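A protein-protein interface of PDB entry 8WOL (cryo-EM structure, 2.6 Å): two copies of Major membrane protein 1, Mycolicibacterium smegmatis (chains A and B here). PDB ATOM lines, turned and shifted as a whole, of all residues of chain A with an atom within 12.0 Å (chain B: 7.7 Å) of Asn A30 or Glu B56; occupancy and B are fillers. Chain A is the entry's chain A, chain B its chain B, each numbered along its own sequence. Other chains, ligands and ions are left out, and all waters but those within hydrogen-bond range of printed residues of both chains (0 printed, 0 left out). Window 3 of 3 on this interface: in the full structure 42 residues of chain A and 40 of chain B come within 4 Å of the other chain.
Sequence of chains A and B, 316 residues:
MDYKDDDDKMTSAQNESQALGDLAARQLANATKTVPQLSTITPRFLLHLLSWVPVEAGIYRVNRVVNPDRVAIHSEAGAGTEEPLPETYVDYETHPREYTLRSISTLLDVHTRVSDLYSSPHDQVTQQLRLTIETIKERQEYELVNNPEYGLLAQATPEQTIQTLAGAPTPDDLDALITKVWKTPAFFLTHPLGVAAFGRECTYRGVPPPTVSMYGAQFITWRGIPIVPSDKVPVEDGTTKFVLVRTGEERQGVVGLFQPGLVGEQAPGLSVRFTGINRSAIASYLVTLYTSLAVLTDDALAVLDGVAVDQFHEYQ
N of Thr A32 sits at hydrogen-bond distance from O of Ile B59, at 3.0 Å.
O of Thr A32 sits at hydrogen-bond distance from N of Arg B61 (2.8 Å).
The backbone carbonyl oxygen (O) of Arg B61 sits at hydrogen-bond distance from the backbone NH (N) of Thr A34 (3.2 Å).
The backbone carbonyl oxygen (O) of Ala A31 is in hydrogen-bond range of the side-chain amino group (NZ) of Lys A33.
NE2 of His A122 lies within hydrogen-bond range of O of Lys A33 (3.4 Å).
The backbone NH (N) of Val B55 is in hydrogen-bond range of the backbone carbonyl oxygen (O) of Phe B258 (3.0 Å).
O of Val B55 sits close to OE1 of Gln B259 (3.2 Å).
The backbone carbonyl oxygen of Glu B56 is in hydrogen-bond range of the side-chain amide nitrogen of Gln B259 (3.3 Å).
Among the printed residues, merely in contact across the chains: Arg A26 with Ile B59 (3.9 Å), Asn A30 with Glu B56 (3.3 Å), Asn A30 with Ala B57 (3.2 Å), Ala A31 with Ile B59 (3.97 Å), Thr A32 with Val B55 (3.9 Å), Thr A32 with Glu B56 (3.6 Å), Thr A32 with Tyr B60 (3.7 Å), Lys A33 with Arg B61 (3.3 Å) and Thr A34 with Tyr B60 (3.3 Å).
No residue of chain B comes within 4 Å of Ala A29.
Of chain B, only Glu B56 (3.3 Å) and Ala B57 (3.2 Å) come within 4 Å of Asn A30.
Of the printed residues of chain B, Ala A31 touches Ile B59 (3.97 Å).
Printed residues of chain B within 4 Å of Thr A32: Val B55, Glu B56, Ile B59, Tyr B60 and Arg B61.
Of the printed residues of chain A, Glu B56 touches Asn A30 and Thr A32.
Of chain A, only Arg A26 (3.9 Å), Ala A31 (3.97 Å) and Thr A32 (3.0 Å) come within 4 Å of Ile B59.
Gln B259 touches none of the printed residues of chain A.
No residue of chain A comes within 4 Å of Pro B260.
The nearest residue of chain B that does not touch Asn A30 is Ile B59 (4.9 Å).
Of the 13 printed residues of chain B, 6 touch a printed residue of chain A.
Hydrophobic or aromatic side chains of chain B that line the printed part of chain A: Val B55, Ala B57, Ile B59 and Tyr B60.
Of the 16 printed residues of chain A, 6 touch a printed residue of chain B.
Along chain A the printed residues that touch a printed residue of chain B span positions 26 to 34.
No position is printed for both chains.
Of the 12 pairs that touch across the chains among the printed residues, none has its exchanged pair printed and touching as well.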
ATOM      1  N   ASP A  22      16.776  12.000   9.015  1.00  0.00           N
ATOM      2  CA  ASP A  22      16.987  12.162   7.581  1.00  0.00           C
ATOM      3  C   ASP A  22      16.269  13.386   7.026  1.00  0.00           C
ATOM      4  O   ASP A  22      16.779  14.041   6.112  1.00  0.00           O
ATOM      5  CB  ASP A  22      16.534  10.904   6.841  1.00  0.00           C
ATOM      6  CG  ASP A  22      17.315   9.675   7.255  1.00  0.00           C
ATOM      7  OD1 ASP A  22      18.379   9.415   6.654  1.00  0.00           O
ATOM      8  OD2 ASP A  22      16.868   8.972   8.183  1.00  0.00           O
ATOM      9  N   LEU A  23      15.082  13.703   7.547  1.00  0.00           N
ATOM     10  CA  LEU A  23      14.322  14.836   7.026  1.00  0.00           C
ATOM     11  C   LEU A  23      15.003  16.159   7.360  1.00  0.00           C
ATOM     12  O   LEU A  23      15.183  17.021   6.487  1.00  0.00           O
ATOM     13  CB  LEU A  23      12.898  14.800   7.582  1.00  0.00           C
ATOM     14  CG  LEU A  23      11.953  15.933   7.175  1.00  0.00           C
ATOM     15  CD1 LEU A  23      11.935  16.102   5.664  1.00  0.00           C
ATOM     16  CD2 LEU A  23      10.553  15.669   7.702  1.00  0.00           C
ATOM     17  N   ALA A  24      15.397  16.334   8.623  1.00  0.00           N
ATOM     18  CA  ALA A  24      16.091  17.554   9.020  1.00  0.00           C
ATOM     19  C   ALA A  24      17.417  17.693   8.284  1.00  0.00           C
ATOM     20  O   ALA A  24      17.817  18.802   7.914  1.00  0.00           O
ATOM     21  CB  ALA A  24      16.310  17.562  10.532  1.00  0.00           C
ATOM     22  N   ALA A  25      18.116  16.577   8.069  1.00  0.00           N
ATOM     23  CA  ALA A  25      19.387  16.624   7.354  1.00  0.00           C
ATOM     24  C   ALA A  25      19.188  16.968   5.883  1.00  0.00           C
ATOM     25  O   ALA A  25      19.967  17.741   5.312  1.00  0.00           O
ATOM     26  CB  ALA A  25      20.119  15.291   7.498  1.00  0.00           C
ATOM     27  N   ARG A  26      18.155  16.406   5.251  1.00  0.00           N
ATOM     28  CA  ARG A  26      17.898  16.695   3.846  1.00  0.00           C
ATOM     29  C   ARG A  26      17.340  18.094   3.646  1.00  0.00           C
ATOM     30  O   ARG A  26      17.361  18.601   2.518  1.00  0.00           O
ATOM     31  CB  ARG A  26      16.942  15.661   3.249  1.00  0.00           C
ATOM     32  CG  ARG A  26      15.481  15.887   3.592  1.00  0.00           C
ATOM     33  CD  ARG A  26      14.577  15.454   2.458  1.00  0.00           C
ATOM     34  NE  ARG A  26      14.672  16.372   1.330  1.00  0.00           N
ATOM     35  CZ  ARG A  26      14.147  16.150   0.133  1.00  0.00           C
ATOM     36  NH1 ARG A  26      13.473  15.043  -0.131  1.00  0.00           N
ATOM     37  NH2 ARG A  26      14.303  17.062  -0.823  1.00  0.00           N
ATOM     38  N   GLN A  27      16.837  18.725   4.709  1.00  0.00           N
ATOM     39  CA  GLN A  27      16.494  20.142   4.631  1.00  0.00           C
ATOM     40  C   GLN A  27      17.682  21.015   4.242  1.00  0.00           C
ATOM     41  O   GLN A  27      17.482  22.179   3.883  1.00  0.00           O
ATOM     42  CB  GLN A  27      15.923  20.623   5.967  1.00  0.00           C
ATOM     43  CG  GLN A  27      14.438  20.341   6.165  1.00  0.00           C
ATOM     44  CD  GLN A  27      13.665  20.300   4.861  1.00  0.00           C
ATOM     45  OE1 GLN A  27      13.193  19.245   4.442  1.00  0.00           O
ATOM     46  NE2 GLN A  27      13.522  21.452   4.220  1.00  0.00           N
ATOM     47  N   LEU A  28      18.905  20.489   4.311  1.00  0.00           N
ATOM     48  CA  LEU A  28      20.109  21.228   3.956  1.00  0.00           C
ATOM     49  C   LEU A  28      20.742  20.761   2.652  1.00  0.00           C
ATOM     50  O   LEU A  28      21.796  21.280   2.274  1.00  0.00           O
ATOM     51  CB  LEU A  28      21.143  21.123   5.085  1.00  0.00           C
ATOM     52  CG  LEU A  28      21.098  22.110   6.253  1.00  0.00           C
ATOM     53  CD1 LEU A  28      19.805  21.988   7.046  1.00  0.00           C
ATOM     54  CD2 LEU A  28      22.297  21.891   7.160  1.00  0.00           C
ATOM     55  N   ALA A  29      20.135  19.805   1.952  1.00  0.00           N
ATOM     56  CA  ALA A  29      20.761  19.150   0.814  1.00  0.00           C
ATOM     57  C   ALA A  29      20.098  19.558  -0.497  1.00  0.00           C
ATOM     58  O   ALA A  29      18.929  19.951  -0.528  1.00  0.00           O
ATOM     59  CB  ALA A  29      20.705  17.627   0.964  1.00  0.00           C
ATOM     60  N   ASN A  30      20.866  19.452  -1.580  1.00  0.00           N
ATOM     61  CA  ASN A  30      20.388  19.766  -2.920  1.00  0.00           C
ATOM     62  C   ASN A  30      19.932  18.497  -3.629  1.00  0.00           C
ATOM     63  O   ASN A  30      20.623  17.476  -3.606  1.00  0.00           O
ATOM     64  CB  ASN A  30      21.491  20.440  -3.738  1.00  0.00           C
ATOM     65  CG  ASN A  30      21.282  21.931  -3.883  1.00  0.00           C
ATOM     66  OD1 ASN A  30      20.157  22.400  -4.056  1.00  0.00           O
ATOM     67  ND2 ASN A  30      22.372  22.688  -3.824  1.00  0.00           N
ATOM     68  N   ALA A  31      18.768  18.570  -4.267  1.00  0.00           N
ATOM     69  CA  ALA A  31      18.251  17.452  -5.042  1.00  0.00           C
ATOM     70  C   ALA A  31      18.726  17.540  -6.488  1.00  0.00           C
ATOM     71  O   ALA A  31      18.946  18.629  -7.027  1.00  0.00           O
ATOM     72  CB  ALA A  31      16.723  17.417  -4.997  1.00  0.00           C
ATOM     73  N   THR A  32      18.884  16.378  -7.115  1.00  0.00           N
ATOM     74  CA  THR A  32      19.263  16.299  -8.520  1.00  0.00           C
ATOM     75  C   THR A  32      17.998  16.311  -9.369  1.00  0.00           C
ATOM     76  O   THR A  32      17.136  15.437  -9.220  1.00  0.00           O
ATOM     77  CB  THR A  32      20.090  15.044  -8.797  1.00  0.00           C
ATOM     78  OG1 THR A  32      21.286  15.073  -8.009  1.00  0.00           O
ATOM     79  CG2 THR A  32      20.464  14.966 -10.268  1.00  0.00           C
ATOM     80  N   LYS A  33      17.891  17.294 -10.257  1.00  0.00           N
ATOM     81  CA  LYS A  33      16.689  17.520 -11.044  1.00  0.00           C
ATOM     82  C   LYS A  33      16.954  17.243 -12.517  1.00  0.00           C
ATOM     83  O   LYS A  33      17.963  17.688 -13.073  1.00  0.00           O
ATOM     84  CB  LYS A  33      16.186  18.955 -10.871  1.00  0.00           C
ATOM     85  CG  LYS A  33      15.771  19.294  -9.453  1.00  0.00           C
ATOM     86  CD  LYS A  33      16.072  20.745  -9.120  1.00  0.00           C
ATOM     87  CE  LYS A  33      15.842  21.023  -7.645  1.00  0.00           C
ATOM     88  NZ  LYS A  33      17.119  21.181  -6.897  1.00  0.00           N
ATOM     89  N   THR A  34      16.043  16.504 -13.139  1.00  0.00           N
ATOM     90  CA  THR A  34      16.115  16.221 -14.563  1.00  0.00           C
ATOM     91  C   THR A  34      15.297  17.238 -15.350  1.00  0.00           C
ATOM     92  O   THR A  34      14.397  17.895 -14.820  1.00  0.00           O
ATOM     93  CB  THR A  34      15.610  14.808 -14.865  1.00  0.00           C
ATOM     94  OG1 THR A  34      14.193  14.748 -14.657  1.00  0.00           O
ATOM     95  CG2 THR A  34      16.290  13.791 -13.962  1.00  0.00           C
ATOM     96  N   SER A 120      17.561  28.689 -12.907  1.00  0.00           N
ATOM     97  CA  SER A 120      18.816  28.100 -12.453  1.00  0.00           C
ATOM     98  C   SER A 120      18.528  26.731 -11.846  1.00  0.00           C
ATOM     99  O   SER A 120      17.654  26.619 -10.970  1.00  0.00           O
ATOM    100  CB  SER A 120      19.522  28.998 -11.435  1.00  0.00           C
ATOM    101  OG  SER A 120      20.918  28.757 -11.428  1.00  0.00           O
ATOM    102  N   PRO A 121      19.242  25.677 -12.266  1.00  0.00           N
ATOM    103  CA  PRO A 121      20.309  25.648 -13.274  1.00  0.00           C
ATOM    104  C   PRO A 121      19.793  25.402 -14.689  1.00  0.00           C
ATOM    105  O   PRO A 121      20.575  25.325 -15.633  1.00  0.00           O
ATOM    106  CB  PRO A 121      21.189  24.495 -12.784  1.00  0.00           C
ATOM    107  CG  PRO A 121      20.197  23.519 -12.206  1.00  0.00           C
ATOM    108  CD  PRO A 121      19.068  24.356 -11.632  1.00  0.00           C
ATOM    109  N   HIS A 122      18.481  25.273 -14.869  1.00  0.00           N
ATOM    110  CA  HIS A 122      17.878  25.040 -16.175  1.00  0.00           C
ATOM    111  C   HIS A 122      17.156  26.298 -16.638  1.00  0.00           C
ATOM    112  O   HIS A 122      16.340  26.858 -15.899  1.00  0.00           O
ATOM    113  CB  HIS A 122      16.895  23.866 -16.127  1.00  0.00           C
ATOM    114  CG  HIS A 122      17.471  22.607 -15.557  1.00  0.00           C
ATOM    115  ND1 HIS A 122      18.666  22.071 -15.987  1.00  0.00           N
ATOM    116  CD2 HIS A 122      17.008  21.769 -14.599  1.00  0.00           C
ATOM    117  CE1 HIS A 122      18.918  20.961 -15.315  1.00  0.00           C
ATOM    118  NE2 HIS A 122      17.926  20.756 -14.466  1.00  0.00           N
ATOM    119  N   VAL B  53      23.873   6.615 -13.089  1.00  0.00           N
ATOM    120  CA  VAL B  53      23.864   8.076 -13.035  1.00  0.00           C
ATOM    121  C   VAL B  53      24.221   8.503 -11.617  1.00  0.00           C
ATOM    122  O   VAL B  53      23.592   8.028 -10.665  1.00  0.00           O
ATOM    123  CB  VAL B  53      22.496   8.655 -13.446  1.00  0.00           C
ATOM    124  CG1 VAL B  53      22.456  10.154 -13.203  1.00  0.00           C
ATOM    125  CG2 VAL B  53      22.204   8.336 -14.901  1.00  0.00           C
ATOM    126  N   PRO B  54      25.211   9.373 -11.432  1.00  0.00           N
ATOM    127  CA  PRO B  54      25.540   9.835 -10.079  1.00  0.00           C
ATOM    128  C   PRO B  54      24.467  10.756  -9.517  1.00  0.00           C
ATOM    129  O   PRO B  54      23.844  11.535 -10.243  1.00  0.00           O
ATOM    130  CB  PRO B  54      26.865  10.580 -10.269  1.00  0.00           C
ATOM    131  CG  PRO B  54      26.875  10.975 -11.707  1.00  0.00           C
ATOM    132  CD  PRO B  54      26.156   9.885 -12.440  1.00  0.00           C
ATOM    133  N   VAL B  55      24.261  10.659  -8.207  1.00  0.00           N
ATOM    134  CA  VAL B  55      23.355  11.533  -7.470  1.00  0.00           C
ATOM    135  C   VAL B  55      24.191  12.273  -6.436  1.00  0.00           C
ATOM    136  O   VAL B  55      24.860  11.643  -5.607  1.00  0.00           O
ATOM    137  CB  VAL B  55      22.217  10.747  -6.802  1.00  0.00           C
ATOM    138  CG1 VAL B  55      21.321  11.680  -6.011  1.00  0.00           C
ATOM    139  CG2 VAL B  55      21.417   9.983  -7.840  1.00  0.00           C
ATOM    140  N   GLU B  56      24.147  13.608  -6.476  1.00  0.00           N
ATOM    141  CA  GLU B  56      25.089  14.398  -5.689  1.00  0.00           C
ATOM    142  C   GLU B  56      24.765  14.385  -4.199  1.00  0.00           C
ATOM    143  O   GLU B  56      25.683  14.461  -3.375  1.00  0.00           O
ATOM    144  CB  GLU B  56      25.135  15.835  -6.214  1.00  0.00           C
ATOM    145  CG  GLU B  56      23.911  16.671  -5.891  1.00  0.00           C
ATOM    146  CD  GLU B  56      24.258  18.111  -5.573  1.00  0.00           C
ATOM    147  OE1 GLU B  56      24.713  18.832  -6.486  1.00  0.00           O
ATOM    148  OE2 GLU B  56      24.069  18.526  -4.411  1.00  0.00           O
ATOM    149  N   ALA B  57      23.485  14.296  -3.825  1.00  0.00           N
ATOM    150  CA  ALA B  57      23.134  14.329  -2.410  1.00  0.00           C
ATOM    151  C   ALA B  57      22.037  13.328  -2.065  1.00  0.00           C
ATOM    152  O   ALA B  57      21.242  13.568  -1.151  1.00  0.00           O
ATOM    153  CB  ALA B  57      22.710  15.734  -1.978  1.00  0.00           C
ATOM    154  N   GLY B  58      21.973  12.210  -2.782  1.00  0.00           N
ATOM    155  CA  GLY B  58      21.093  11.122  -2.413  1.00  0.00           C
ATOM    156  C   GLY B  58      19.637  11.282  -2.794  1.00  0.00           C
ATOM    157  O   GLY B  58      18.835  10.397  -2.473  1.00  0.00           O
ATOM    158  N   ILE B  59      19.261  12.372  -3.460  1.00  0.00           N
ATOM    159  CA  ILE B  59      17.883  12.600  -3.878  1.00  0.00           C
ATOM    160  C   ILE B  59      17.867  12.802  -5.386  1.00  0.00           C
ATOM    161  O   ILE B  59      18.645  13.600  -5.919  1.00  0.00           O
ATOM    162  CB  ILE B  59      17.253  13.813  -3.165  1.00  0.00           C
ATOM    163  CG1 ILE B  59      17.569  13.784  -1.667  1.00  0.00           C
ATOM    164  CG2 ILE B  59      15.749  13.849  -3.403  1.00  0.00           C
ATOM    165  CD1 ILE B  59      16.636  12.910  -0.857  1.00  0.00           C
ATOM    166  N   TYR B  60      16.981  12.080  -6.069  1.00  0.00           N
ATOM    167  CA  TYR B  60      16.842  12.158  -7.518  1.00  0.00           C
ATOM    168  C   TYR B  60      15.392  12.476  -7.845  1.00  0.00           C
ATOM    169  O   TYR B  60      14.489  11.731  -7.452  1.00  0.00           O
ATOM    170  CB  TYR B  60      17.269  10.845  -8.181  1.00  0.00           C
ATOM    171  CG  TYR B  60      17.561  10.955  -9.660  1.00  0.00           C
ATOM    172  CD1 TYR B  60      18.707  11.591 -10.114  1.00  0.00           C
ATOM    173  CD2 TYR B  60      16.697  10.409 -10.600  1.00  0.00           C
ATOM    174  CE1 TYR B  60      18.982  11.688 -11.462  1.00  0.00           C
ATOM    175  CE2 TYR B  60      16.964  10.500 -11.950  1.00  0.00           C
ATOM    176  CZ  TYR B  60      18.108  11.141 -12.375  1.00  0.00           C
ATOM    177  OH  TYR B  60      18.379  11.236 -13.720  1.00  0.00           O
ATOM    178  N   ARG B  61      15.171  13.573  -8.565  1.00  0.00           N
ATOM    179  CA  ARG B  61      13.834  14.028  -8.926  1.00  0.00           C
ATOM    180  C   ARG B  61      13.654  13.906 -10.433  1.00  0.00           C
ATOM    181  O   ARG B  61      14.470  14.425 -11.203  1.00  0.00           O
ATOM    182  CB  ARG B  61      13.605  15.470  -8.473  1.00  0.00           C
ATOM    183  CG  ARG B  61      12.194  15.975  -8.720  1.00  0.00           C
ATOM    184  CD  ARG B  61      12.094  17.477  -8.527  1.00  0.00           C
ATOM    185  NE  ARG B  61      12.175  17.856  -7.122  1.00  0.00           N
ATOM    186  CZ  ARG B  61      12.465  19.076  -6.691  1.00  0.00           C
ATOM    187  NH1 ARG B  61      12.690  20.072  -7.533  1.00  0.00           N
ATOM    188  NH2 ARG B  61      12.530  19.303  -5.383  1.00  0.00           N
ATOM    189  N   LEU B 101      18.340   7.216  -2.257  1.00  0.00           N
ATOM    190  CA  LEU B 101      19.143   6.002  -2.237  1.00  0.00           C
ATOM    191  C   LEU B 101      18.923   5.221  -0.947  1.00  0.00           C
ATOM    192  O   LEU B 101      18.771   5.800   0.134  1.00  0.00           O
ATOM    193  CB  LEU B 101      20.622   6.347  -2.397  1.00  0.00           C
ATOM    194  CG  LEU B 101      20.988   7.140  -3.653  1.00  0.00           C
ATOM    195  CD1 LEU B 101      22.445   7.566  -3.624  1.00  0.00           C
ATOM    196  CD2 LEU B 101      20.693   6.330  -4.903  1.00  0.00           C
ATOM    197  N   PHE B 258      23.624   5.982  -7.897  1.00  0.00           N
ATOM    198  CA  PHE B 258      24.630   5.701  -6.883  1.00  0.00           C
ATOM    199  C   PHE B 258      25.174   7.016  -6.340  1.00  0.00           C
ATOM    200  O   PHE B 258      25.034   8.073  -6.959  1.00  0.00           O
ATOM    201  CB  PHE B 258      25.765   4.831  -7.439  1.00  0.00           C
ATOM    202  CG  PHE B 258      26.681   5.554  -8.381  1.00  0.00           C
ATOM    203  CD1 PHE B 258      26.316   5.756  -9.701  1.00  0.00           C
ATOM    204  CD2 PHE B 258      27.910   6.028  -7.950  1.00  0.00           C
ATOM    205  CE1 PHE B 258      27.154   6.417 -10.572  1.00  0.00           C
ATOM    206  CE2 PHE B 258      28.752   6.692  -8.818  1.00  0.00           C
ATOM    207  CZ  PHE B 258      28.373   6.887 -10.131  1.00  0.00           C
ATOM    208  N   GLN B 259      25.801   6.934  -5.166  1.00  0.00           N
ATOM    209  CA  GLN B 259      26.360   8.106  -4.505  1.00  0.00           C
ATOM    210  C   GLN B 259      27.866   8.137  -4.699  1.00  0.00           C
ATOM    211  O   GLN B 259      28.560   7.225  -4.221  1.00  0.00           O
ATOM    212  CB  GLN B 259      26.021   8.097  -3.020  1.00  0.00           C
ATOM    213  CG  GLN B 259      26.670   9.220  -2.224  1.00  0.00           C
ATOM    214  CD  GLN B 259      26.108  10.585  -2.572  1.00  0.00           C
ATOM    215  OE1 GLN B 259      24.905  10.816  -2.477  1.00  0.00           O
ATOM    216  NE2 GLN B 259      26.981  11.497  -2.978  1.00  0.00           N
ATOM    217  N   PRO B 260      28.413   9.137  -5.380  1.00  0.00           N
ATOM    218  CA  PRO B 260      29.863   9.222  -5.563  1.00  0.00           C
ATOM    219  C   PRO B 260      30.542   9.946  -4.404  1.00  0.00           C
ATOM    220  O   PRO B 260      29.903  10.601  -3.579  1.00  0.00           O
ATOM    221  CB  PRO B 260      29.997  10.027  -6.861  1.00  0.00           C
ATOM    222  CG  PRO B 260      28.794  10.909  -6.871  1.00  0.00           C
ATOM    223  CD  PRO B 260      27.700  10.206  -6.099  1.00  0.00           C
